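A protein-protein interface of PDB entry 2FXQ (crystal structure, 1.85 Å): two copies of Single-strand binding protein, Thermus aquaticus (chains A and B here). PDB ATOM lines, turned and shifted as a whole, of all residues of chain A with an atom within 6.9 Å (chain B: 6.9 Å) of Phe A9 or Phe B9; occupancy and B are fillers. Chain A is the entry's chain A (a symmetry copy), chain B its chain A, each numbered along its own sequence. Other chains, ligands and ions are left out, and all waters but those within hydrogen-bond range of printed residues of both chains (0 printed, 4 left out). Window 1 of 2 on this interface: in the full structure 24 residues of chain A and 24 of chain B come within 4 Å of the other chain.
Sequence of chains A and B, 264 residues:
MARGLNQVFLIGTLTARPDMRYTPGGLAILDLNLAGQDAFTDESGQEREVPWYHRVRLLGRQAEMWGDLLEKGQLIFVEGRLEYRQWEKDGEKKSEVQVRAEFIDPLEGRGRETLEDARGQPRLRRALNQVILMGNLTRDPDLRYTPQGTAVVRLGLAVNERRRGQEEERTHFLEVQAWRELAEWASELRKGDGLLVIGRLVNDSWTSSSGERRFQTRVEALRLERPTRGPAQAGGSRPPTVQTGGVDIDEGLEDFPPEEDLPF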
ATOM      1  N   GLN A   7      26.167   0.517   5.642  1.00  0.00           N
ATOM      2  CA  GLN A   7      24.915   0.975   5.016  1.00  0.00           C
ATOM      3  C   GLN A   7      23.940  -0.135   4.985  1.00  0.00           C
ATOM      4  O   GLN A   7      24.303  -1.244   4.645  1.00  0.00           O
ATOM      5  CB  GLN A   7      25.168   1.396   3.526  1.00  0.00           C
ATOM      6  CG  GLN A   7      26.306   2.482   3.458  1.00  0.00           C
ATOM      7  CD  GLN A   7      26.656   2.878   1.996  1.00  0.00           C
ATOM      8  OE1 GLN A   7      26.662   2.019   1.121  1.00  0.00           O
ATOM      9  NE2 GLN A   7      26.906   4.169   1.741  1.00  0.00           N
ATOM     10  N   VAL A   8      22.678   0.167   5.304  1.00  0.00           N
ATOM     11  CA  VAL A   8      21.618  -0.827   5.340  1.00  0.00           C
ATOM     12  C   VAL A   8      20.426  -0.249   4.559  1.00  0.00           C
ATOM     13  O   VAL A   8      20.127   0.968   4.684  1.00  0.00           O
ATOM     14  CB  VAL A   8      21.107  -1.039   6.830  1.00  0.00           C
ATOM     15  CG1 VAL A   8      19.934  -2.069   6.854  1.00  0.00           C
ATOM     16  CG2 VAL A   8      22.279  -1.406   7.750  1.00  0.00           C
ATOM     17  N   PHE A   9      19.752  -1.097   3.759  1.00  0.00           N
ATOM     18  CA  PHE A   9      18.557  -0.705   2.979  1.00  0.00           C
ATOM     19  C   PHE A   9      17.567  -1.782   3.230  1.00  0.00           C
ATOM     20  O   PHE A   9      17.907  -2.980   3.102  1.00  0.00           O
ATOM     21  CB  PHE A   9      18.898  -0.679   1.450  1.00  0.00           C
ATOM     22  CG  PHE A   9      20.148   0.100   1.129  1.00  0.00           C
ATOM     23  CD1 PHE A   9      20.068   1.416   0.699  1.00  0.00           C
ATOM     24  CD2 PHE A   9      21.436  -0.477   1.300  1.00  0.00           C
ATOM     25  CE1 PHE A   9      21.250   2.189   0.481  1.00  0.00           C
ATOM     26  CE2 PHE A   9      22.612   0.300   1.036  1.00  0.00           C
ATOM     27  CZ  PHE A   9      22.509   1.604   0.649  1.00  0.00           C
ATOM     28  N   LEU A  10      16.346  -1.428   3.657  1.00  0.00           N
ATOM     29  CA  LEU A  10      15.387  -2.451   4.047  1.00  0.00           C
ATOM     30  C   LEU A  10      14.056  -1.949   3.642  1.00  0.00           C
ATOM     31  O   LEU A  10      13.788  -0.717   3.729  1.00  0.00           O
ATOM     32  CB  LEU A  10      15.276  -2.507   5.588  1.00  0.00           C
ATOM     33  CG  LEU A  10      16.190  -3.283   6.443  1.00  0.00           C
ATOM     34  CD1 LEU A  10      15.709  -3.105   7.923  1.00  0.00           C
ATOM     35  CD2 LEU A  10      16.216  -4.754   5.929  1.00  0.00           C
ATOM     36  N   ILE A  11      13.225  -2.833   3.150  1.00  0.00           N
ATOM     37  CA  ILE A  11      11.792  -2.540   3.199  1.00  0.00           C
ATOM     38  C   ILE A  11      11.197  -3.681   4.009  1.00  0.00           C
ATOM     39  O   ILE A  11      11.444  -4.853   3.700  1.00  0.00           O
ATOM     40  CB  ILE A  11      11.169  -2.568   1.760  1.00  0.00           C
ATOM     41  CG1 ILE A  11      11.771  -1.431   0.907  1.00  0.00           C
ATOM     42  CG2 ILE A  11       9.579  -2.532   1.840  1.00  0.00           C
ATOM     43  CD1 ILE A  11      11.369  -1.525  -0.637  1.00  0.00           C
ATOM     44  N   PHE A  77      10.195   1.854   4.034  1.00  0.00           N
ATOM     45  CA  PHE A  77      11.526   1.818   3.438  1.00  0.00           C
ATOM     46  C   PHE A  77      12.490   2.541   4.384  1.00  0.00           C
ATOM     47  O   PHE A  77      12.191   3.605   4.914  1.00  0.00           O
ATOM     48  CB  PHE A  77      11.464   2.553   2.051  1.00  0.00           C
ATOM     49  CG  PHE A  77      12.811   2.783   1.429  1.00  0.00           C
ATOM     50  CD1 PHE A  77      13.539   1.726   1.026  1.00  0.00           C
ATOM     51  CD2 PHE A  77      13.322   4.058   1.253  1.00  0.00           C
ATOM     52  CE1 PHE A  77      14.827   1.900   0.412  1.00  0.00           C
ATOM     53  CE2 PHE A  77      14.591   4.275   0.627  1.00  0.00           C
ATOM     54  CZ  PHE A  77      15.322   3.187   0.195  1.00  0.00           C
ATOM     55  N   VAL A  78      13.646   1.934   4.658  1.00  0.00           N
ATOM     56  CA  VAL A  78      14.598   2.472   5.627  1.00  0.00           C
ATOM     57  C   VAL A  78      15.963   2.521   4.963  1.00  0.00           C
ATOM     58  O   VAL A  78      16.330   1.575   4.273  1.00  0.00           O
ATOM     59  CB  VAL A  78      14.732   1.428   6.821  1.00  0.00           C
ATOM     60  CG1 VAL A  78      15.750   1.924   7.816  1.00  0.00           C
ATOM     61  CG2 VAL A  78      13.361   1.181   7.449  1.00  0.00           C
ATOM     62  N   GLU A  79      16.698   3.606   5.147  1.00  0.00           N
ATOM     63  CA  GLU A  79      18.140   3.558   4.957  1.00  0.00           C
ATOM     64  C   GLU A  79      18.831   3.946   6.255  1.00  0.00           C
ATOM     65  O   GLU A  79      18.400   4.861   6.969  1.00  0.00           O
ATOM     66  CB  GLU A  79      18.599   4.528   3.832  1.00  0.00           C
ATOM     67  CG  GLU A  79      18.070   4.112   2.451  1.00  0.00           C
ATOM     68  CD  GLU A  79      18.740   4.844   1.281  1.00  0.00           C
ATOM     69  OE1 GLU A  79      18.437   4.500   0.089  1.00  0.00           O
ATOM     70  OE2 GLU A  79      19.639   5.662   1.556  1.00  0.00           O
ATOM     71  N   GLY A  80      19.900   3.238   6.581  1.00  0.00           N
ATOM     72  CA  GLY A  80      20.553   3.554   7.839  1.00  0.00           C
ATOM     73  C   GLY A  80      21.873   2.840   7.940  1.00  0.00           C
ATOM     74  O   GLY A  80      22.520   2.567   6.915  1.00  0.00           O
ATOM     75  N   VAL A  99      19.347  -1.438  13.537  1.00  0.00           N
ATOM     76  CA  VAL A  99      19.562  -0.518  12.414  1.00  0.00           C
ATOM     77  C   VAL A  99      19.260   0.845  13.011  1.00  0.00           C
ATOM     78  O   VAL A  99      18.164   1.044  13.528  1.00  0.00           O
ATOM     79  CB  VAL A  99      18.584  -0.783  11.293  1.00  0.00           C
ATOM     80  CG1 VAL A  99      18.728   0.329  10.173  1.00  0.00           C
ATOM     81  CG2 VAL A  99      18.811  -2.217  10.779  1.00  0.00           C
ATOM     82  N   LEU A 128      13.807  -6.260  -0.356  1.00  0.00           N
ATOM     83  CA  LEU A 128      14.881  -5.335  -0.010  1.00  0.00           C
ATOM     84  C   LEU A 128      15.363  -5.594   1.468  1.00  0.00           C
ATOM     85  O   LEU A 128      14.735  -5.269   2.484  1.00  0.00           O
ATOM     86  CB  LEU A 128      14.554  -3.865  -0.366  1.00  0.00           C
ATOM     87  CG  LEU A 128      15.737  -2.878  -0.400  1.00  0.00           C
ATOM     88  CD1 LEU A 128      16.577  -2.984  -1.680  1.00  0.00           C
ATOM     89  CD2 LEU A 128      15.367  -1.430  -0.171  1.00  0.00           C
ATOM     90  N   ASN A 129      16.518  -6.242   1.541  1.00  0.00           N
ATOM     91  CA  ASN A 129      17.209  -6.369   2.789  1.00  0.00           C
ATOM     92  C   ASN A 129      18.642  -6.449   2.325  1.00  0.00           C
ATOM     93  O   ASN A 129      19.089  -7.496   1.862  1.00  0.00           O
ATOM     94  CB  ASN A 129      16.739  -7.654   3.432  1.00  0.00           C
ATOM     95  CG  ASN A 129      17.621  -8.100   4.542  1.00  0.00           C
ATOM     96  OD1 ASN A 129      18.522  -7.364   4.918  1.00  0.00           O
ATOM     97  ND2 ASN A 129      17.324  -9.280   5.136  1.00  0.00           N
ATOM     98  N   GLN A 130      19.330  -5.324   2.326  1.00  0.00           N
ATOM     99  CA  GLN A 130      20.696  -5.257   1.816  1.00  0.00           C
ATOM    100  C   GLN A 130      21.602  -4.549   2.799  1.00  0.00           C
ATOM    101  O   GLN A 130      21.223  -3.511   3.383  1.00  0.00           O
ATOM    102  CB  GLN A 130      20.763  -4.476   0.474  1.00  0.00           C
ATOM    103  CG  GLN A 130      22.280  -4.323  -0.091  1.00  0.00           C
ATOM    104  CD  GLN A 130      22.419  -4.212  -1.632  1.00  0.00           C
ATOM    105  OE1 GLN A 130      22.427  -5.232  -2.361  1.00  0.00           O
ATOM    106  NE2 GLN A 130      22.540  -2.975  -2.117  1.00  0.00           N
ATOM    107  N   VAL A 131      22.820  -5.088   2.999  1.00  0.00           N
ATOM    108  CA  VAL A 131      23.767  -4.401   3.807  1.00  0.00           C
ATOM    109  C   VAL A 131      25.067  -4.257   2.982  1.00  0.00           C
ATOM    110  O   VAL A 131      25.430  -5.176   2.249  1.00  0.00           O
ATOM    111  CB  VAL A 131      24.088  -5.326   5.052  1.00  0.00           C
ATOM    112  CG1 VAL A 131      25.225  -4.690   5.862  1.00  0.00           C
ATOM    113  CG2 VAL A 131      22.793  -5.534   5.959  1.00  0.00           C
ATOM    114  N   ILE A 132      25.729  -3.084   3.076  1.00  0.00           N
ATOM    115  CA  ILE A 132      27.043  -2.903   2.446  1.00  0.00           C
ATOM    116  C   ILE A 132      27.988  -2.533   3.594  1.00  0.00           C
ATOM    117  O   ILE A 132      27.746  -1.541   4.319  1.00  0.00           O
ATOM    118  CB  ILE A 132      27.015  -1.827   1.389  1.00  0.00           C
ATOM    119  CG1 ILE A 132      26.033  -2.238   0.268  1.00  0.00           C
ATOM    120  CG2 ILE A 132      28.476  -1.657   0.784  1.00  0.00           C
ATOM    121  CD1 ILE A 132      25.901  -1.110  -0.897  1.00  0.00           C
ATOM    122  N   GLN B   7      20.291   7.267  -6.142  1.00  0.00           N
ATOM    123  CA  GLN B   7      21.448   6.504  -5.643  1.00  0.00           C
ATOM    124  C   GLN B   7      21.724   5.370  -6.549  1.00  0.00           C
ATOM    125  O   GLN B   7      20.804   4.689  -6.956  1.00  0.00           O
ATOM    126  CB  GLN B   7      21.135   5.891  -4.233  1.00  0.00           C
ATOM    127  CG  GLN B   7      20.689   7.026  -3.238  1.00  0.00           C
ATOM    128  CD  GLN B   7      20.287   6.465  -1.845  1.00  0.00           C
ATOM    129  OE1 GLN B   7      19.683   5.401  -1.772  1.00  0.00           O
ATOM    130  NE2 GLN B   7      20.656   7.159  -0.761  1.00  0.00           N
ATOM    131  N   VAL B   8      23.006   5.134  -6.840  1.00  0.00           N
ATOM    132  CA  VAL B   8      23.425   4.068  -7.736  1.00  0.00           C
ATOM    133  C   VAL B   8      24.559   3.302  -7.034  1.00  0.00           C
ATOM    134  O   VAL B   8      25.434   3.937  -6.386  1.00  0.00           O
ATOM    135  CB  VAL B   8      24.059   4.675  -9.061  1.00  0.00           C
ATOM    136  CG1 VAL B   8      24.553   3.526  -9.995  1.00  0.00           C
ATOM    137  CG2 VAL B   8      23.074   5.644  -9.730  1.00  0.00           C
ATOM    138  N   PHE B   9      24.551   1.961  -7.147  1.00  0.00           N
ATOM    139  CA  PHE B   9      25.596   1.088  -6.568  1.00  0.00           C
ATOM    140  C   PHE B   9      25.958   0.150  -7.660  1.00  0.00           C
ATOM    141  O   PHE B   9      25.057  -0.454  -8.285  1.00  0.00           O
ATOM    142  CB  PHE B   9      25.007   0.266  -5.372  1.00  0.00           C
ATOM    143  CG  PHE B   9      24.264   1.114  -4.371  1.00  0.00           C
ATOM    144  CD1 PHE B   9      24.888   1.547  -3.211  1.00  0.00           C
ATOM    145  CD2 PHE B   9      22.925   1.527  -4.610  1.00  0.00           C
ATOM    146  CE1 PHE B   9      24.221   2.426  -2.303  1.00  0.00           C
ATOM    147  CE2 PHE B   9      22.255   2.375  -3.669  1.00  0.00           C
ATOM    148  CZ  PHE B   9      22.902   2.817  -2.552  1.00  0.00           C
ATOM    149  N   LEU B  10      27.254   0.036  -7.987  1.00  0.00           N
ATOM    150  CA  LEU B  10      27.645  -0.765  -9.139  1.00  0.00           C
ATOM    151  C   LEU B  10      28.936  -1.395  -8.787  1.00  0.00           C
ATOM    152  O   LEU B  10      29.784  -0.764  -8.096  1.00  0.00           O
ATOM    153  CB  LEU B  10      28.027   0.160 -10.316  1.00  0.00           C
ATOM    154  CG  LEU B  10      27.047   0.725 -11.260  1.00  0.00           C
ATOM    155  CD1 LEU B  10      27.845   1.564 -12.316  1.00  0.00           C
ATOM    156  CD2 LEU B  10      26.198  -0.442 -11.848  1.00  0.00           C
ATOM    157  N   ILE B  11      29.107  -2.632  -9.181  1.00  0.00           N
ATOM    158  CA  ILE B  11      30.474  -3.134  -9.317  1.00  0.00           C
ATOM    159  C   ILE B  11      30.585  -3.547 -10.776  1.00  0.00           C
ATOM    160  O   ILE B  11      29.738  -4.301 -11.271  1.00  0.00           O
ATOM    161  CB  ILE B  11      30.694  -4.401  -8.418  1.00  0.00           C
ATOM    162  CG1 ILE B  11      30.566  -4.014  -6.929  1.00  0.00           C
ATOM    163  CG2 ILE B  11      32.075  -5.106  -8.778  1.00  0.00           C
ATOM    164  CD1 ILE B  11      30.545  -5.279  -5.952  1.00  0.00           C
ATOM    165  N   PHE B  77      34.151  -0.850  -7.363  1.00  0.00           N
ATOM    166  CA  PHE B  77      32.884  -0.610  -6.683  1.00  0.00           C
ATOM    167  C   PHE B  77      32.614   0.899  -6.697  1.00  0.00           C
ATOM    168  O   PHE B  77      33.497   1.710  -6.444  1.00  0.00           O
ATOM    169  CB  PHE B  77      33.013  -1.129  -5.206  1.00  0.00           C
ATOM    170  CG  PHE B  77      31.857  -0.746  -4.328  1.00  0.00           C
ATOM    171  CD1 PHE B  77      30.639  -1.259  -4.581  1.00  0.00           C
ATOM    172  CD2 PHE B  77      32.012   0.120  -3.258  1.00  0.00           C
ATOM    173  CE1 PHE B  77      29.508  -0.933  -3.757  1.00  0.00           C
ATOM    174  CE2 PHE B  77      30.916   0.455  -2.402  1.00  0.00           C
ATOM    175  CZ  PHE B  77      29.674  -0.094  -2.654  1.00  0.00           C
ATOM    176  N   VAL B  78      31.393   1.297  -7.058  1.00  0.00           N
ATOM    177  CA  VAL B  78      31.049   2.708  -7.214  1.00  0.00           C
ATOM    178  C   VAL B  78      29.780   2.969  -6.420  1.00  0.00           C
ATOM    179  O   VAL B  78      28.865   2.153  -6.465  1.00  0.00           O
ATOM    180  CB  VAL B  78      30.668   2.959  -8.739  1.00  0.00           C
ATOM    181  CG1 VAL B  78      30.252   4.396  -8.927  1.00  0.00           C
ATOM    182  CG2 VAL B  78      31.837   2.559  -9.637  1.00  0.00           C
ATOM    183  N   GLU B  79      29.727   4.072  -5.691  1.00  0.00           N
ATOM    184  CA  GLU B  79      28.443   4.627  -5.290  1.00  0.00           C
ATOM    185  C   GLU B  79      28.313   6.039  -5.835  1.00  0.00           C
ATOM    186  O   GLU B  79      29.272   6.822  -5.841  1.00  0.00           O
ATOM    187  CB  GLU B  79      28.299   4.668  -3.742  1.00  0.00           C
ATOM    188  CG  GLU B  79      28.261   3.264  -3.121  1.00  0.00           C
ATOM    189  CD  GLU B  79      27.812   3.243  -1.654  1.00  0.00           C
ATOM    190  OE1 GLU B  79      27.657   2.115  -1.077  1.00  0.00           O
ATOM    191  OE2 GLU B  79      27.507   4.334  -1.132  1.00  0.00           O
ATOM    192  N   GLY B  80      27.127   6.372  -6.318  1.00  0.00           N
ATOM    193  CA  GLY B  80      26.985   7.699  -6.891  1.00  0.00           C
ATOM    194  C   GLY B  80      25.538   8.003  -7.162  1.00  0.00           C
ATOM    195  O   GLY B  80      24.646   7.491  -6.465  1.00  0.00           O
ATOM    196  N   VAL B  99      26.727   7.989 -14.551  1.00  0.00           N
ATOM    197  CA  VAL B  99      26.765   7.884 -13.088  1.00  0.00           C
ATOM    198  C   VAL B  99      27.812   8.909 -12.688  1.00  0.00           C
ATOM    199  O   VAL B  99      28.943   8.826 -13.157  1.00  0.00           O
ATOM    200  CB  VAL B  99      27.236   6.516 -12.649  1.00  0.00           C
ATOM    201  CG1 VAL B  99      27.429   6.489 -11.076  1.00  0.00           C
ATOM    202  CG2 VAL B  99      26.235   5.468 -13.171  1.00  0.00           C
ATOM    203  N   LEU B 128      26.216  -6.614  -8.768  1.00  0.00           N
ATOM    204  CA  LEU B 128      25.830  -5.330  -8.191  1.00  0.00           C
ATOM    205  C   LEU B 128      25.598  -4.272  -9.336  1.00  0.00           C
ATOM    206  O   LEU B 128      26.496  -3.726  -9.988  1.00  0.00           O
ATOM    207  CB  LEU B 128      26.755  -4.882  -7.034  1.00  0.00           C
ATOM    208  CG  LEU B 128      26.229  -3.759  -6.120  1.00  0.00           C
ATOM    209  CD1 LEU B 128      25.204  -4.249  -5.088  1.00  0.00           C
ATOM    210  CD2 LEU B 128      27.300  -2.960  -5.411  1.00  0.00           C
ATOM    211  N   ASN B 129      24.316  -4.030  -9.578  1.00  0.00           N
ATOM    212  CA  ASN B 129      23.924  -2.945 -10.426  1.00  0.00           C
ATOM    213  C   ASN B 129      22.575  -2.592  -9.848  1.00  0.00           C
ATOM    214  O   ASN B 129      21.589  -3.277 -10.109  1.00  0.00           O
ATOM    215  CB  ASN B 129      23.823  -3.489 -11.832  1.00  0.00           C
ATOM    216  CG  ASN B 129      23.085  -2.583 -12.751  1.00  0.00           C
ATOM    217  OD1 ASN B 129      22.759  -1.473 -12.356  1.00  0.00           O
ATOM    218  ND2 ASN B 129      22.880  -3.014 -14.018  1.00  0.00           N
ATOM    219  N   GLN B 130      22.544  -1.610  -8.969  1.00  0.00           N
ATOM    220  CA  GLN B 130      21.315  -1.237  -8.276  1.00  0.00           C
ATOM    221  C   GLN B 130      21.095   0.258  -8.339  1.00  0.00           C
ATOM    222  O   GLN B 130      22.044   1.051  -8.159  1.00  0.00           O
ATOM    223  CB  GLN B 130      21.367  -1.638  -6.776  1.00  0.00           C
ATOM    224  CG  GLN B 130      20.040  -1.177  -5.954  1.00  0.00           C
ATOM    225  CD  GLN B 130      19.661  -2.058  -4.734  1.00  0.00           C
ATOM    226  OE1 GLN B 130      19.006  -3.117  -4.874  1.00  0.00           O
ATOM    227  NE2 GLN B 130      20.066  -1.608  -3.546  1.00  0.00           N
ATOM    228  N   VAL B 131      19.840   0.677  -8.589  1.00  0.00           N
ATOM    229  CA  VAL B 131      19.540   2.067  -8.531  1.00  0.00           C
ATOM    230  C   VAL B 131      18.339   2.244  -7.571  1.00  0.00           C
ATOM    231  O   VAL B 131      17.431   1.414  -7.569  1.00  0.00           O
ATOM    232  CB  VAL B 131      19.069   2.511  -9.976  1.00  0.00           C
ATOM    233  CG1 VAL B 131      18.583   3.965  -9.914  1.00  0.00           C
ATOM    234  CG2 VAL B 131      20.250   2.352 -11.036  1.00  0.00           C
ATOM    235  N   ILE B 132      18.372   3.303  -6.734  1.00  0.00           N
ATOM    236  CA  ILE B 132      17.219   3.636  -5.889  1.00  0.00           C
ATOM    237  C   ILE B 132      16.834   5.066  -6.286  1.00  0.00           C
ATOM    238  O   ILE B 132      17.674   5.991  -6.210  1.00  0.00           O
ATOM    239  CB  ILE B 132      17.554   3.546  -4.421  1.00  0.00           C
ATOM    240  CG1 ILE B 132      17.955   2.093  -4.078  1.00  0.00           C
ATOM    241  CG2 ILE B 132      16.275   3.961  -3.571  1.00  0.00           C
ATOM    242  CD1 ILE B 132      18.381   1.909  -2.519  1.00  0.00           C
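Printed residues of chain B that touch a printed residue of chain A: Gln B7, Phe B9, Phe B77, Glu B79, Gln B130 and Ile B132.
Hydrophobic or aromatic side chains of chain B that line the printed part of chain A: Phe B9, Phe B77 and Ile B132.
Of the 15 printed residues of chain A, 6 touch a printed residue of chain B.
Printed residues of chain A that touch a printed residue of chain B: Gln A7, Phe A9, Phe A77, Glu A79, Gln A130 and Ile A132.
Among the printed residues, 10 pairs touch across the chains.
Among the printed residues, no Asp or Glu carboxylate lies within 4 Å of a Lys or Arg side-chain nitrogen of the other chain.
The side-chain carboxylate of Glu B79 lies close to the side-chain amide oxygen of Gln A7 (2.4 Å).
The side-chain amide oxygen (OE1) of Gln B7 sits close to the side-chain carboxylate (OE1) of Glu A79 (2.4 Å).
The side-chain amide nitrogen (NE2) of Gln A130 sits close to the side-chain amide nitrogen (NE2) of Gln B130, at 3.2 Å.
Phe A9 touches Phe B9 (CZ to CZ, 3.4 Å).
Ile B132 touches Phe A9 (CD1 to CD1, 3.7 Å).
Phe A77 touches Ile B132.
Glu A79 touches Ile B132 (OE1 to CD1, 3.7 Å).
Ile A132 touches Phe B9.
Phe B77 touches Ile A132 (CZ to CG2, 3.96 Å).
OE1 of Glu B79 touches CD1 of Ile A132, 3.7 Å away.
Gln A7 touches Glu B79, and with the chains exchanged Glu A79 touches Gln B7.
Phe B9 touches its own counterpart, Phe A9.
Glu A79 touches Ile B132, and with the chains exchanged Ile A132 touches Glu B79.
Gln B130 touches its own counterpart, Gln A130.
Positions printed for both chains: 7, 8, 9, 10, 11, 77, 78, 79, 80, 99, 128, 129, 130, 131 and 132.
Of the 10 pairs that touch across the chains among the printed residues, 10 have their exchanged pair printed and touching as well.
Of the printed residues of chain B, Phe A9 touches Phe B9 (3.4 Å) and Ile B132 (3.7 Å).
Printed residues of chain B within 4 Å of Glu A79: Gln B7 (2.4 Å) and Ile B132 (3.7 Å).
Asn A129 touches none of the printed residues of chain B.
Of the printed residues of chain B, Gln A130 touches Gln B130.
Printed residues of chain B within 4 Å of Ile A132: Phe B9 (3.7 Å), Phe B77 (3.96 Å) and Glu B79 (3.7 Å).
Of chain A, only Phe A9 and Ile A132 come within 4 Å of Phe B9.
Printed residues of chain A within 4 Å of Phe B77: Ile A132.
Printed residues of chain A within 4 Å of Gln B130: Gln A130 (3.2 Å).
The nearest residue of chain A that does not touch Phe B9 is Gln A7 (4.2 Å).
The nearest printed residue of chain B that does not touch Ile A132 is Leu B128 (5.1 Å).
The backbone carbonyl oxygen (O) of Gln B7 sits at hydrogen-bond distance from the backbone NH (N) of Ile B132 (2.8 Å).
O of Phe B9 is in hydrogen-bond range of N of Gln B130, 2.8 Å away.
N of Ile A132 sits at hydrogen-bond distance from O of Gln A7 (2.8 Å).
O of Phe A9 sits at hydrogen-bond distance from N of Gln A130, 2.8 Å away.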
